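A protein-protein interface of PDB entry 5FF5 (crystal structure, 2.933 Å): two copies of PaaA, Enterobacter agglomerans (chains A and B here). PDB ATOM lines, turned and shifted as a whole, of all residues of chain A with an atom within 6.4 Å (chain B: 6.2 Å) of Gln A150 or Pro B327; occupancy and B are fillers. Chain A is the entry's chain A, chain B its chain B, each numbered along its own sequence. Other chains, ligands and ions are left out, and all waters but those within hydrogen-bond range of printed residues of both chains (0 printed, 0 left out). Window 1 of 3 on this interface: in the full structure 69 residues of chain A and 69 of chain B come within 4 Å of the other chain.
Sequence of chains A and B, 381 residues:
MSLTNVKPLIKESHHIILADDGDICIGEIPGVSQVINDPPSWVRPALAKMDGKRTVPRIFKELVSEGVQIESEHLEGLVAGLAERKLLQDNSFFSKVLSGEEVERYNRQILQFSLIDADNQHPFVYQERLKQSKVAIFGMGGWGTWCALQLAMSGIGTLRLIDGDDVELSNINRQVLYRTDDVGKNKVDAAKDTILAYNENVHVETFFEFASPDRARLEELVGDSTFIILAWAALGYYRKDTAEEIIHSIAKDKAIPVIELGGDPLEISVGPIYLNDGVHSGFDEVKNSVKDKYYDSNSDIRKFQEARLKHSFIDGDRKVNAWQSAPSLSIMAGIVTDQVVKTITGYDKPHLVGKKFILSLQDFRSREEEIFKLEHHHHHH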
ATOM      1  N   GLN A 109      11.465 -34.903  -3.857  1.00  0.00           N
ATOM      2  CA  GLN A 109      11.493 -33.659  -4.616  1.00  0.00           C
ATOM      3  C   GLN A 109      12.735 -33.672  -5.492  1.00  0.00           C
ATOM      4  O   GLN A 109      12.752 -33.104  -6.578  1.00  0.00           O
ATOM      5  CB  GLN A 109      11.483 -32.436  -3.731  1.00  0.00           C
ATOM      6  CG  GLN A 109      12.819 -32.118  -3.153  1.00  0.00           C
ATOM      7  CD  GLN A 109      12.781 -30.914  -2.272  1.00  0.00           C
ATOM      8  OE1 GLN A 109      11.768 -30.611  -1.645  1.00  0.00           O
ATOM      9  NE2 GLN A 109      13.882 -30.189  -2.243  1.00  0.00           N
ATOM     10  N   GLN A 112      11.620 -35.215  -8.548  1.00  0.00           N
ATOM     11  CA  GLN A 112      10.919 -34.265  -9.388  1.00  0.00           C
ATOM     12  C   GLN A 112      11.863 -33.410 -10.221  1.00  0.00           C
ATOM     13  O   GLN A 112      11.556 -33.118 -11.371  1.00  0.00           O
ATOM     14  CB  GLN A 112      10.025 -33.394  -8.530  1.00  0.00           C
ATOM     15  CG  GLN A 112       9.382 -32.257  -9.262  1.00  0.00           C
ATOM     16  CD  GLN A 112       8.539 -31.412  -8.326  1.00  0.00           C
ATOM     17  OE1 GLN A 112       7.828 -31.945  -7.463  1.00  0.00           O
ATOM     18  NE2 GLN A 112       8.626 -30.089  -8.472  1.00  0.00           N
ATOM     19  N   THR A 145       4.200 -16.659   7.033  1.00  0.00           N
ATOM     20  CA  THR A 145       4.443 -17.916   7.745  1.00  0.00           C
ATOM     21  C   THR A 145       4.416 -19.143   6.838  1.00  0.00           C
ATOM     22  O   THR A 145       5.153 -20.098   7.059  1.00  0.00           O
ATOM     23  CB  THR A 145       3.395 -18.141   8.859  1.00  0.00           C
ATOM     24  OG1 THR A 145       2.079 -17.921   8.342  1.00  0.00           O
ATOM     25  CG2 THR A 145       3.622 -17.196  10.014  1.00  0.00           C
ATOM     26  N   TRP A 146       3.572 -19.126   5.814  1.00  0.00           N
ATOM     27  CA  TRP A 146       3.466 -20.277   4.924  1.00  0.00           C
ATOM     28  C   TRP A 146       4.654 -20.368   3.998  1.00  0.00           C
ATOM     29  O   TRP A 146       5.104 -21.465   3.684  1.00  0.00           O
ATOM     30  CB  TRP A 146       2.174 -20.219   4.123  1.00  0.00           C
ATOM     31  CG  TRP A 146       0.976 -20.484   4.952  1.00  0.00           C
ATOM     32  CD1 TRP A 146       0.271 -19.584   5.686  1.00  0.00           C
ATOM     33  CD2 TRP A 146       0.338 -21.743   5.141  1.00  0.00           C
ATOM     34  NE1 TRP A 146      -0.767 -20.205   6.326  1.00  0.00           N
ATOM     35  CE2 TRP A 146      -0.750 -21.535   6.006  1.00  0.00           C
ATOM     36  CE3 TRP A 146       0.573 -23.035   4.648  1.00  0.00           C
ATOM     37  CZ2 TRP A 146      -1.597 -22.556   6.394  1.00  0.00           C
ATOM     38  CZ3 TRP A 146      -0.262 -24.051   5.043  1.00  0.00           C
ATOM     39  CH2 TRP A 146      -1.339 -23.807   5.905  1.00  0.00           C
ATOM     40  N   CYS A 147       5.163 -19.221   3.564  1.00  0.00           N
ATOM     41  CA  CYS A 147       6.335 -19.218   2.700  1.00  0.00           C
ATOM     42  C   CYS A 147       7.577 -19.728   3.427  1.00  0.00           C
ATOM     43  O   CYS A 147       8.364 -20.485   2.862  1.00  0.00           O
ATOM     44  CB  CYS A 147       6.614 -17.830   2.143  1.00  0.00           C
ATOM     45  SG  CYS A 147       5.497 -17.275   0.851  1.00  0.00           S
ATOM     46  N   ALA A 148       7.775 -19.286   4.665  1.00  0.00           N
ATOM     47  CA  ALA A 148       8.910 -19.755   5.445  1.00  0.00           C
ATOM     48  C   ALA A 148       8.859 -21.271   5.567  1.00  0.00           C
ATOM     49  O   ALA A 148       9.860 -21.972   5.356  1.00  0.00           O
ATOM     50  CB  ALA A 148       8.922 -19.109   6.823  1.00  0.00           C
ATOM     51  N   LEU A 149       7.670 -21.762   5.899  1.00  0.00           N
ATOM     52  CA  LEU A 149       7.475 -23.167   6.151  1.00  0.00           C
ATOM     53  C   LEU A 149       7.874 -24.024   4.971  1.00  0.00           C
ATOM     54  O   LEU A 149       8.763 -24.864   5.090  1.00  0.00           O
ATOM     55  CB  LEU A 149       6.026 -23.454   6.499  1.00  0.00           C
ATOM     56  CG  LEU A 149       5.808 -24.934   6.811  1.00  0.00           C
ATOM     57  CD1 LEU A 149       6.857 -25.441   7.803  1.00  0.00           C
ATOM     58  CD2 LEU A 149       4.414 -25.176   7.307  1.00  0.00           C
ATOM     59  N   GLN A 150       7.206 -23.816   3.836  1.00  0.00           N
ATOM     60  CA  GLN A 150       7.405 -24.675   2.667  1.00  0.00           C
ATOM     61  C   GLN A 150       8.817 -24.559   2.125  1.00  0.00           C
ATOM     62  O   GLN A 150       9.370 -25.541   1.620  1.00  0.00           O
ATOM     63  CB  GLN A 150       6.381 -24.346   1.573  1.00  0.00           C
ATOM     64  CG  GLN A 150       4.967 -24.802   1.898  1.00  0.00           C
ATOM     65  CD  GLN A 150       3.953 -24.381   0.857  1.00  0.00           C
ATOM     66  OE1 GLN A 150       4.292 -24.166  -0.303  1.00  0.00           O
ATOM     67  NE2 GLN A 150       2.697 -24.270   1.266  1.00  0.00           N
ATOM     68  N   LEU A 151       9.406 -23.379   2.278  1.00  0.00           N
ATOM     69  CA  LEU A 151      10.800 -23.168   1.941  1.00  0.00           C
ATOM     70  C   LEU A 151      11.712 -23.971   2.872  1.00  0.00           C
ATOM     71  O   LEU A 151      12.681 -24.596   2.430  1.00  0.00           O
ATOM     72  CB  LEU A 151      11.137 -21.685   2.026  1.00  0.00           C
ATOM     73  CG  LEU A 151      10.683 -20.808   0.863  1.00  0.00           C
ATOM     74  CD1 LEU A 151      10.604 -19.331   1.272  1.00  0.00           C
ATOM     75  CD2 LEU A 151      11.653 -20.993  -0.298  1.00  0.00           C
ATOM     76  N   ALA A 152      11.404 -23.978   4.160  1.00  0.00           N
ATOM     77  CA  ALA A 152      12.222 -24.748   5.087  1.00  0.00           C
ATOM     78  C   ALA A 152      12.119 -26.243   4.756  1.00  0.00           C
ATOM     79  O   ALA A 152      13.132 -26.956   4.695  1.00  0.00           O
ATOM     80  CB  ALA A 152      11.805 -24.478   6.521  1.00  0.00           C
ATOM     81  N   MET A 153      10.891 -26.710   4.528  1.00  0.00           N
ATOM     82  CA  MET A 153      10.663 -28.107   4.185  1.00  0.00           C
ATOM     83  C   MET A 153      11.422 -28.497   2.911  1.00  0.00           C
ATOM     84  O   MET A 153      11.929 -29.617   2.786  1.00  0.00           O
ATOM     85  CB  MET A 153       9.166 -28.385   4.016  1.00  0.00           C
ATOM     86  CG  MET A 153       8.344 -28.169   5.277  1.00  0.00           C
ATOM     87  SD  MET A 153       6.397 -28.397   5.027  1.00  0.00           S
ATOM     88  CE  MET A 153       6.207 -30.187   5.779  1.00  0.00           C
ATOM     89  N   SER A 154      11.516 -27.557   1.979  1.00  0.00           N
ATOM     90  CA  SER A 154      12.066 -27.839   0.673  1.00  0.00           C
ATOM     91  C   SER A 154      13.591 -27.850   0.700  1.00  0.00           C
ATOM     92  O   SER A 154      14.244 -28.135  -0.314  1.00  0.00           O
ATOM     93  CB  SER A 154      11.550 -26.813  -0.305  1.00  0.00           C
ATOM     94  OG  SER A 154      10.147 -26.940  -0.385  1.00  0.00           O
ATOM     95  N   GLY A 155      14.161 -27.554   1.865  1.00  0.00           N
ATOM     96  CA  GLY A 155      15.596 -27.596   2.012  1.00  0.00           C
ATOM     97  C   GLY A 155      16.291 -26.299   1.664  1.00  0.00           C
ATOM     98  O   GLY A 155      17.447 -26.331   1.275  1.00  0.00           O
ATOM     99  N   ILE A 156      15.594 -25.167   1.759  1.00  0.00           N
ATOM    100  CA  ILE A 156      16.231 -23.850   1.600  1.00  0.00           C
ATOM    101  C   ILE A 156      17.420 -23.747   2.539  1.00  0.00           C
ATOM    102  O   ILE A 156      17.397 -24.268   3.648  1.00  0.00           O
ATOM    103  CB  ILE A 156      15.270 -22.675   1.905  1.00  0.00           C
ATOM    104  CG1 ILE A 156      15.614 -21.458   1.061  1.00  0.00           C
ATOM    105  CG2 ILE A 156      15.266 -22.329   3.385  1.00  0.00           C
ATOM    106  CD1 ILE A 156      15.176 -21.592  -0.372  1.00  0.00           C
ATOM    107  N   LEU A 329      -3.907 -18.579   1.940  1.00  0.00           N
ATOM    108  CA  LEU A 329      -2.476 -18.434   2.160  1.00  0.00           C
ATOM    109  C   LEU A 329      -1.679 -19.613   1.609  1.00  0.00           C
ATOM    110  O   LEU A 329      -0.583 -19.427   1.066  1.00  0.00           O
ATOM    111  CB  LEU A 329      -2.183 -18.273   3.649  1.00  0.00           C
ATOM    112  CG  LEU A 329      -2.878 -17.138   4.398  1.00  0.00           C
ATOM    113  CD1 LEU A 329      -2.426 -17.158   5.849  1.00  0.00           C
ATOM    114  CD2 LEU A 329      -2.570 -15.815   3.763  1.00  0.00           C
ATOM    115  N   SER A 330      -2.209 -20.825   1.764  1.00  0.00           N
ATOM    116  CA  SER A 330      -1.467 -22.010   1.329  1.00  0.00           C
ATOM    117  C   SER A 330      -1.318 -22.008  -0.185  1.00  0.00           C
ATOM    118  O   SER A 330      -0.236 -22.314  -0.718  1.00  0.00           O
ATOM    119  CB  SER A 330      -2.151 -23.310   1.778  1.00  0.00           C
ATOM    120  OG  SER A 330      -3.361 -23.053   2.466  1.00  0.00           O
ATOM    121  N   ILE A 331      -2.392 -21.631  -0.874  1.00  0.00           N
ATOM    122  CA  ILE A 331      -2.333 -21.548  -2.316  1.00  0.00           C
ATOM    123  C   ILE A 331      -1.250 -20.555  -2.713  1.00  0.00           C
ATOM    124  O   ILE A 331      -0.407 -20.857  -3.556  1.00  0.00           O
ATOM    125  CB  ILE A 331      -3.662 -21.119  -2.920  1.00  0.00           C
ATOM    126  CG1 ILE A 331      -4.734 -22.152  -2.643  1.00  0.00           C
ATOM    127  CG2 ILE A 331      -3.521 -20.965  -4.411  1.00  0.00           C
ATOM    128  CD1 ILE A 331      -5.992 -21.876  -3.374  1.00  0.00           C
ATOM    129  N   ALA A 333       1.359 -19.339  -0.976  1.00  0.00           N
ATOM    130  CA  ALA A 333       2.727 -19.722  -0.628  1.00  0.00           C
ATOM    131  C   ALA A 333       3.255 -20.868  -1.500  1.00  0.00           C
ATOM    132  O   ALA A 333       4.462 -20.954  -1.762  1.00  0.00           O
ATOM    133  CB  ALA A 333       2.809 -20.100   0.820  1.00  0.00           C
ATOM    134  N   GLY A 334       2.352 -21.750  -1.926  1.00  0.00           N
ATOM    135  CA  GLY A 334       2.703 -22.876  -2.770  1.00  0.00           C
ATOM    136  C   GLY A 334       3.037 -22.468  -4.189  1.00  0.00           C
ATOM    137  O   GLY A 334       3.929 -23.034  -4.805  1.00  0.00           O
ATOM    138  N   ILE A 335       2.276 -21.528  -4.736  1.00  0.00           N
ATOM    139  CA  ILE A 335       2.615 -20.935  -6.017  1.00  0.00           C
ATOM    140  C   ILE A 335       3.965 -20.219  -5.922  1.00  0.00           C
ATOM    141  O   ILE A 335       4.825 -20.371  -6.785  1.00  0.00           O
ATOM    142  CB  ILE A 335       1.548 -19.947  -6.465  1.00  0.00           C
ATOM    143  CG1 ILE A 335       0.181 -20.610  -6.440  1.00  0.00           C
ATOM    144  CG2 ILE A 335       1.869 -19.397  -7.834  1.00  0.00           C
ATOM    145  CD1 ILE A 335      -0.920 -19.729  -6.948  1.00  0.00           C
ATOM    146  N   THR A 337       6.389 -20.672  -3.614  1.00  0.00           N
ATOM    147  CA  THR A 337       7.489 -21.553  -3.288  1.00  0.00           C
ATOM    148  C   THR A 337       7.939 -22.330  -4.521  1.00  0.00           C
ATOM    149  O   THR A 337       9.143 -22.398  -4.807  1.00  0.00           O
ATOM    150  CB  THR A 337       7.092 -22.513  -2.175  1.00  0.00           C
ATOM    151  OG1 THR A 337       6.647 -21.748  -1.054  1.00  0.00           O
ATOM    152  CG2 THR A 337       8.267 -23.388  -1.768  1.00  0.00           C
ATOM    153  N   ASP A 338       6.974 -22.879  -5.262  1.00  0.00           N
ATOM    154  CA  ASP A 338       7.275 -23.567  -6.508  1.00  0.00           C
ATOM    155  C   ASP A 338       8.025 -22.644  -7.471  1.00  0.00           C
ATOM    156  O   ASP A 338       9.032 -23.052  -8.053  1.00  0.00           O
ATOM    157  CB  ASP A 338       6.008 -24.103  -7.159  1.00  0.00           C
ATOM    158  CG  ASP A 338       6.294 -24.871  -8.464  1.00  0.00           C
ATOM    159  OD1 ASP A 338       6.772 -26.034  -8.377  1.00  0.00           O
ATOM    160  OD2 ASP A 338       6.009 -24.341  -9.570  1.00  0.00           O
ATOM    161  N   VAL A 341      11.519 -21.944  -6.103  1.00  0.00           N
ATOM    162  CA  VAL A 341      12.376 -23.110  -6.231  1.00  0.00           C
ATOM    163  C   VAL A 341      12.828 -23.323  -7.668  1.00  0.00           C
ATOM    164  O   VAL A 341      14.011 -23.545  -7.925  1.00  0.00           O
ATOM    165  CB  VAL A 341      11.695 -24.369  -5.713  1.00  0.00           C
ATOM    166  CG1 VAL A 341      12.445 -25.601  -6.188  1.00  0.00           C
ATOM    167  CG2 VAL A 341      11.665 -24.327  -4.197  1.00  0.00           C
ATOM    168  N   TRP B 146      -2.300 -31.941   4.695  1.00  0.00           N
ATOM    169  CA  TRP B 146      -2.525 -30.521   4.467  1.00  0.00           C
ATOM    170  C   TRP B 146      -3.999 -30.214   4.641  1.00  0.00           C
ATOM    171  O   TRP B 146      -4.359 -29.173   5.147  1.00  0.00           O
ATOM    172  CB  TRP B 146      -2.050 -30.101   3.073  1.00  0.00           C
ATOM    173  CG  TRP B 146      -0.563 -30.115   2.922  1.00  0.00           C
ATOM    174  CD1 TRP B 146       0.204 -31.182   2.595  1.00  0.00           C
ATOM    175  CD2 TRP B 146       0.342 -29.009   3.091  1.00  0.00           C
ATOM    176  NE1 TRP B 146       1.529 -30.821   2.548  1.00  0.00           N
ATOM    177  CE2 TRP B 146       1.639 -29.494   2.847  1.00  0.00           C
ATOM    178  CE3 TRP B 146       0.179 -27.660   3.428  1.00  0.00           C
ATOM    179  CZ2 TRP B 146       2.766 -28.687   2.931  1.00  0.00           C
ATOM    180  CZ3 TRP B 146       1.308 -26.856   3.506  1.00  0.00           C
ATOM    181  CH2 TRP B 146       2.584 -27.375   3.260  1.00  0.00           C
ATOM    182  N   ASN B 173       9.605 -33.853   3.834  1.00  0.00           N
ATOM    183  CA  ASN B 173       9.662 -32.688   2.938  1.00  0.00           C
ATOM    184  C   ASN B 173       8.294 -32.155   2.466  1.00  0.00           C
ATOM    185  O   ASN B 173       8.190 -30.999   2.059  1.00  0.00           O
ATOM    186  CB  ASN B 173      10.535 -32.947   1.703  1.00  0.00           C
ATOM    187  CG  ASN B 173       9.834 -33.789   0.635  1.00  0.00           C
ATOM    188  OD1 ASN B 173       9.046 -34.680   0.945  1.00  0.00           O
ATOM    189  ND2 ASN B 173      10.092 -33.475  -0.635  1.00  0.00           N
ATOM    190  N   SER B 325       6.468 -33.071  -4.212  1.00  0.00           N
ATOM    191  CA  SER B 325       7.018 -32.047  -3.298  1.00  0.00           C
ATOM    192  C   SER B 325       5.911 -31.150  -2.737  1.00  0.00           C
ATOM    193  O   SER B 325       4.800 -31.117  -3.272  1.00  0.00           O
ATOM    194  CB  SER B 325       8.076 -31.188  -3.983  1.00  0.00           C
ATOM    195  OG  SER B 325       7.489 -30.417  -5.009  1.00  0.00           O
ATOM    196  N   ALA B 326       6.238 -30.383  -1.700  1.00  0.00           N
ATOM    197  CA  ALA B 326       5.224 -29.682  -0.913  1.00  0.00           C
ATOM    198  C   ALA B 326       4.333 -28.693  -1.680  1.00  0.00           C
ATOM    199  O   ALA B 326       3.126 -28.675  -1.457  1.00  0.00           O
ATOM    200  CB  ALA B 326       5.887 -28.965   0.245  1.00  0.00           C
ATOM    201  N   PRO B 327       4.903 -27.877  -2.580  1.00  0.00           N
ATOM    202  CA  PRO B 327       4.123 -26.812  -3.232  1.00  0.00           C
ATOM    203  C   PRO B 327       2.787 -27.222  -3.872  1.00  0.00           C
ATOM    204  O   PRO B 327       1.781 -26.549  -3.683  1.00  0.00           O
ATOM    205  CB  PRO B 327       5.069 -26.329  -4.325  1.00  0.00           C
ATOM    206  CG  PRO B 327       6.401 -26.587  -3.792  1.00  0.00           C
ATOM    207  CD  PRO B 327       6.313 -27.847  -2.993  1.00  0.00           C
ATOM    208  N   SER B 328       2.784 -28.326  -4.604  1.00  0.00           N
ATOM    209  CA  SER B 328       1.602 -28.793  -5.322  1.00  0.00           C
ATOM    210  C   SER B 328       0.516 -29.266  -4.372  1.00  0.00           C
ATOM    211  O   SER B 328      -0.670 -29.056  -4.620  1.00  0.00           O
ATOM    212  CB  SER B 328       2.010 -29.913  -6.266  1.00  0.00           C
ATOM    213  OG  SER B 328       3.432 -30.023  -6.279  1.00  0.00           O
ATOM    214  N   LEU B 329       0.918 -29.879  -3.266  1.00  0.00           N
ATOM    215  CA  LEU B 329      -0.059 -30.370  -2.314  1.00  0.00           C
ATOM    216  C   LEU B 329      -0.766 -29.237  -1.588  1.00  0.00           C
ATOM    217  O   LEU B 329      -1.968 -29.306  -1.361  1.00  0.00           O
ATOM    218  CB  LEU B 329       0.582 -31.278  -1.277  1.00  0.00           C
ATOM    219  CG  LEU B 329       1.336 -32.535  -1.651  1.00  0.00           C
ATOM    220  CD1 LEU B 329       1.821 -33.142  -0.370  1.00  0.00           C
ATOM    221  CD2 LEU B 329       0.434 -33.508  -2.367  1.00  0.00           C
ATOM    222  N   SER B 330      -0.033 -28.199  -1.207  1.00  0.00           N
ATOM    223  CA  SER B 330      -0.653 -27.126  -0.439  1.00  0.00           C
ATOM    224  C   SER B 330      -1.667 -26.360  -1.282  1.00  0.00           C
ATOM    225  O   SER B 330      -2.728 -25.983  -0.782  1.00  0.00           O
ATOM    226  CB  SER B 330       0.401 -26.178   0.138  1.00  0.00           C
ATOM    227  OG  SER B 330       1.114 -25.518  -0.881  1.00  0.00           O
ATOM    228  N   ILE B 331      -1.350 -26.145  -2.555  1.00  0.00           N
ATOM    229  CA  ILE B 331      -2.274 -25.461  -3.445  1.00  0.00           C
ATOM    230  C   ILE B 331      -3.602 -26.205  -3.552  1.00  0.00           C
ATOM    231  O   ILE B 331      -4.653 -25.599  -3.365  1.00  0.00           O
ATOM    232  CB  ILE B 331      -1.713 -25.297  -4.848  1.00  0.00           C
ATOM    233  CG1 ILE B 331      -0.411 -24.507  -4.811  1.00  0.00           C
ATOM    234  CG2 ILE B 331      -2.724 -24.630  -5.724  1.00  0.00           C
ATOM    235  CD1 ILE B 331       0.107 -24.126  -6.179  1.00  0.00           C
ATOM    236  N   MET B 332      -3.591 -27.507  -3.845  1.00  0.00           N
ATOM    237  CA  MET B 332      -4.881 -28.171  -3.948  1.00  0.00           C
ATOM    238  C   MET B 332      -5.499 -28.386  -2.574  1.00  0.00           C
ATOM    239  O   MET B 332      -6.703 -28.260  -2.429  1.00  0.00           O
ATOM    240  CB  MET B 332      -4.801 -29.484  -4.747  1.00  0.00           C
ATOM    241  CG  MET B 332      -3.957 -30.609  -4.213  1.00  0.00           C
ATOM    242  SD  MET B 332      -3.822 -32.058  -5.565  1.00  0.00           S
ATOM    243  CE  MET B 332      -1.891 -32.334  -5.480  1.00  0.00           C
ATOM    244  N   LEU B 361       0.798 -26.149 -13.161  1.00  0.00           N
ATOM    245  CA  LEU B 361       1.688 -25.351 -12.318  1.00  0.00           C
ATOM    246  C   LEU B 361       2.914 -24.906 -13.095  1.00  0.00           C
ATOM    247  O   LEU B 361       3.805 -24.266 -12.539  1.00  0.00           O
ATOM    248  CB  LEU B 361       2.149 -26.118 -11.079  1.00  0.00           C
ATOM    249  CG  LEU B 361       1.110 -26.568 -10.068  1.00  0.00           C
ATOM    250  CD1 LEU B 361       1.824 -27.074  -8.822  1.00  0.00           C
ATOM    251  CD2 LEU B 361       0.099 -25.474  -9.760  1.00  0.00           C
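OG of Ser B330 sits at hydrogen-bond distance from O of Ser A330. ND2 of Asn B173 is in hydrogen-bond range of OE1 of Gln A109. OE1 of Gln A112 lies within hydrogen-bond range of OG of Ser B325, 2.9 Å away. NE2 of Gln A150 sits at hydrogen-bond distance from OG of Ser B330 (2.9 Å).
The backbone carbonyl oxygen of Ser A154 sits at hydrogen-bond distance from the side-chain amide nitrogen of Gln A109, at 2.8 Å. OE1 of Gln A150 sits close to N of Gly A334 (3.5 Å). The backbone carbonyl oxygen (O) of Gln A150 lies within hydrogen-bond range of the side-chain hydroxyl (OG) of Ser A154 (2.6 Å). The backbone carbonyl oxygen of Ser B325 lies within hydrogen-bond range of the side-chain hydroxyl of Ser B328, 3.5 Å away. The backbone carbonyl oxygen (O) of Pro B327 sits at hydrogen-bond distance from the side-chain hydroxyl (OG) of Ser B330 (3.1 Å). The side-chain amide oxygen (OE1) of Gln A150 sits at hydrogen-bond distance from the side-chain hydroxyl (OG1) of Thr A337, 3.5 Å away.
Gln A109 touches Ser B325 (CB to CB, 3.6 Å). CZ3 of Trp A146 touches CZ3 of Trp B146, 3.6 Å away. Gln A150 touches Trp B146 (NE2 to CH2, 3.7 Å). OE1 of Gln A150 touches CA of Pro B327, at 3.95 Å. Asn B173 touches Met A153 (O to CB, 3.4 Å). Ile B331 touches Ile A331. CD1 of Ile B331 touches C of Gly A334, 3.9 Å away. Ile B331 touches Ile A335. Pro B327 touches Asp A338. Asp A338 touches Leu B361 (OD2 to O, 3.7 Å).
Of chain B, only Trp B146 (3.7 Å), Pro B327 (3.95 Å) and Ser B330 (2.9 Å) come within 4 Å of Gln A150. Of the printed residues of chain A, Pro B327 touches Gln A150 (3.95 Å), Gly A334 (3.5 Å) and Asp A338 (3.7 Å). Printed residues of chain B within 4 Å of Ile A331: Ile B331. Of the printed residues of chain B, Gln A109 touches Asn B173 and Ser B325. Ser A154 touches none of the printed residues of chain B. Thr A337 touches none of the printed residues of chain B. The nearest residue of chain A that does not touch Pro B327 is Thr A337 (4.2 Å).
Of the 11 printed residues of chain B, 7 touch a printed residue of chain A. Hydrophobic or aromatic side chains of chain B that line the printed part of chain A: Trp B146, Pro B327 and Ile B331. Of the 23 printed residues of chain A, 10 touch a printed residue of chain B. Printed residues of chain A that touch a printed residue of chain B: Gln A109, Gln A112, Trp A146, Gln A150, Met A153, Ser A330, Ile A331, Gly A334, Ile A335 and Asp A338. Hydrophobic or aromatic side chains of chain A that line the printed part of chain B: Trp A146, Met A153, Ile A331 and Ile A335.
Trp A146 touches its own counterpart, Trp B146. Ser B330 touches its own counterpart, Ser A330. Ile B331 touches its own counterpart, Ile A331. Positions printed for both chains: 146, 329, 330 and 331. Of the 16 pairs that touch across the chains among the printed residues, 3 have their exchanged pair printed and touching as well.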
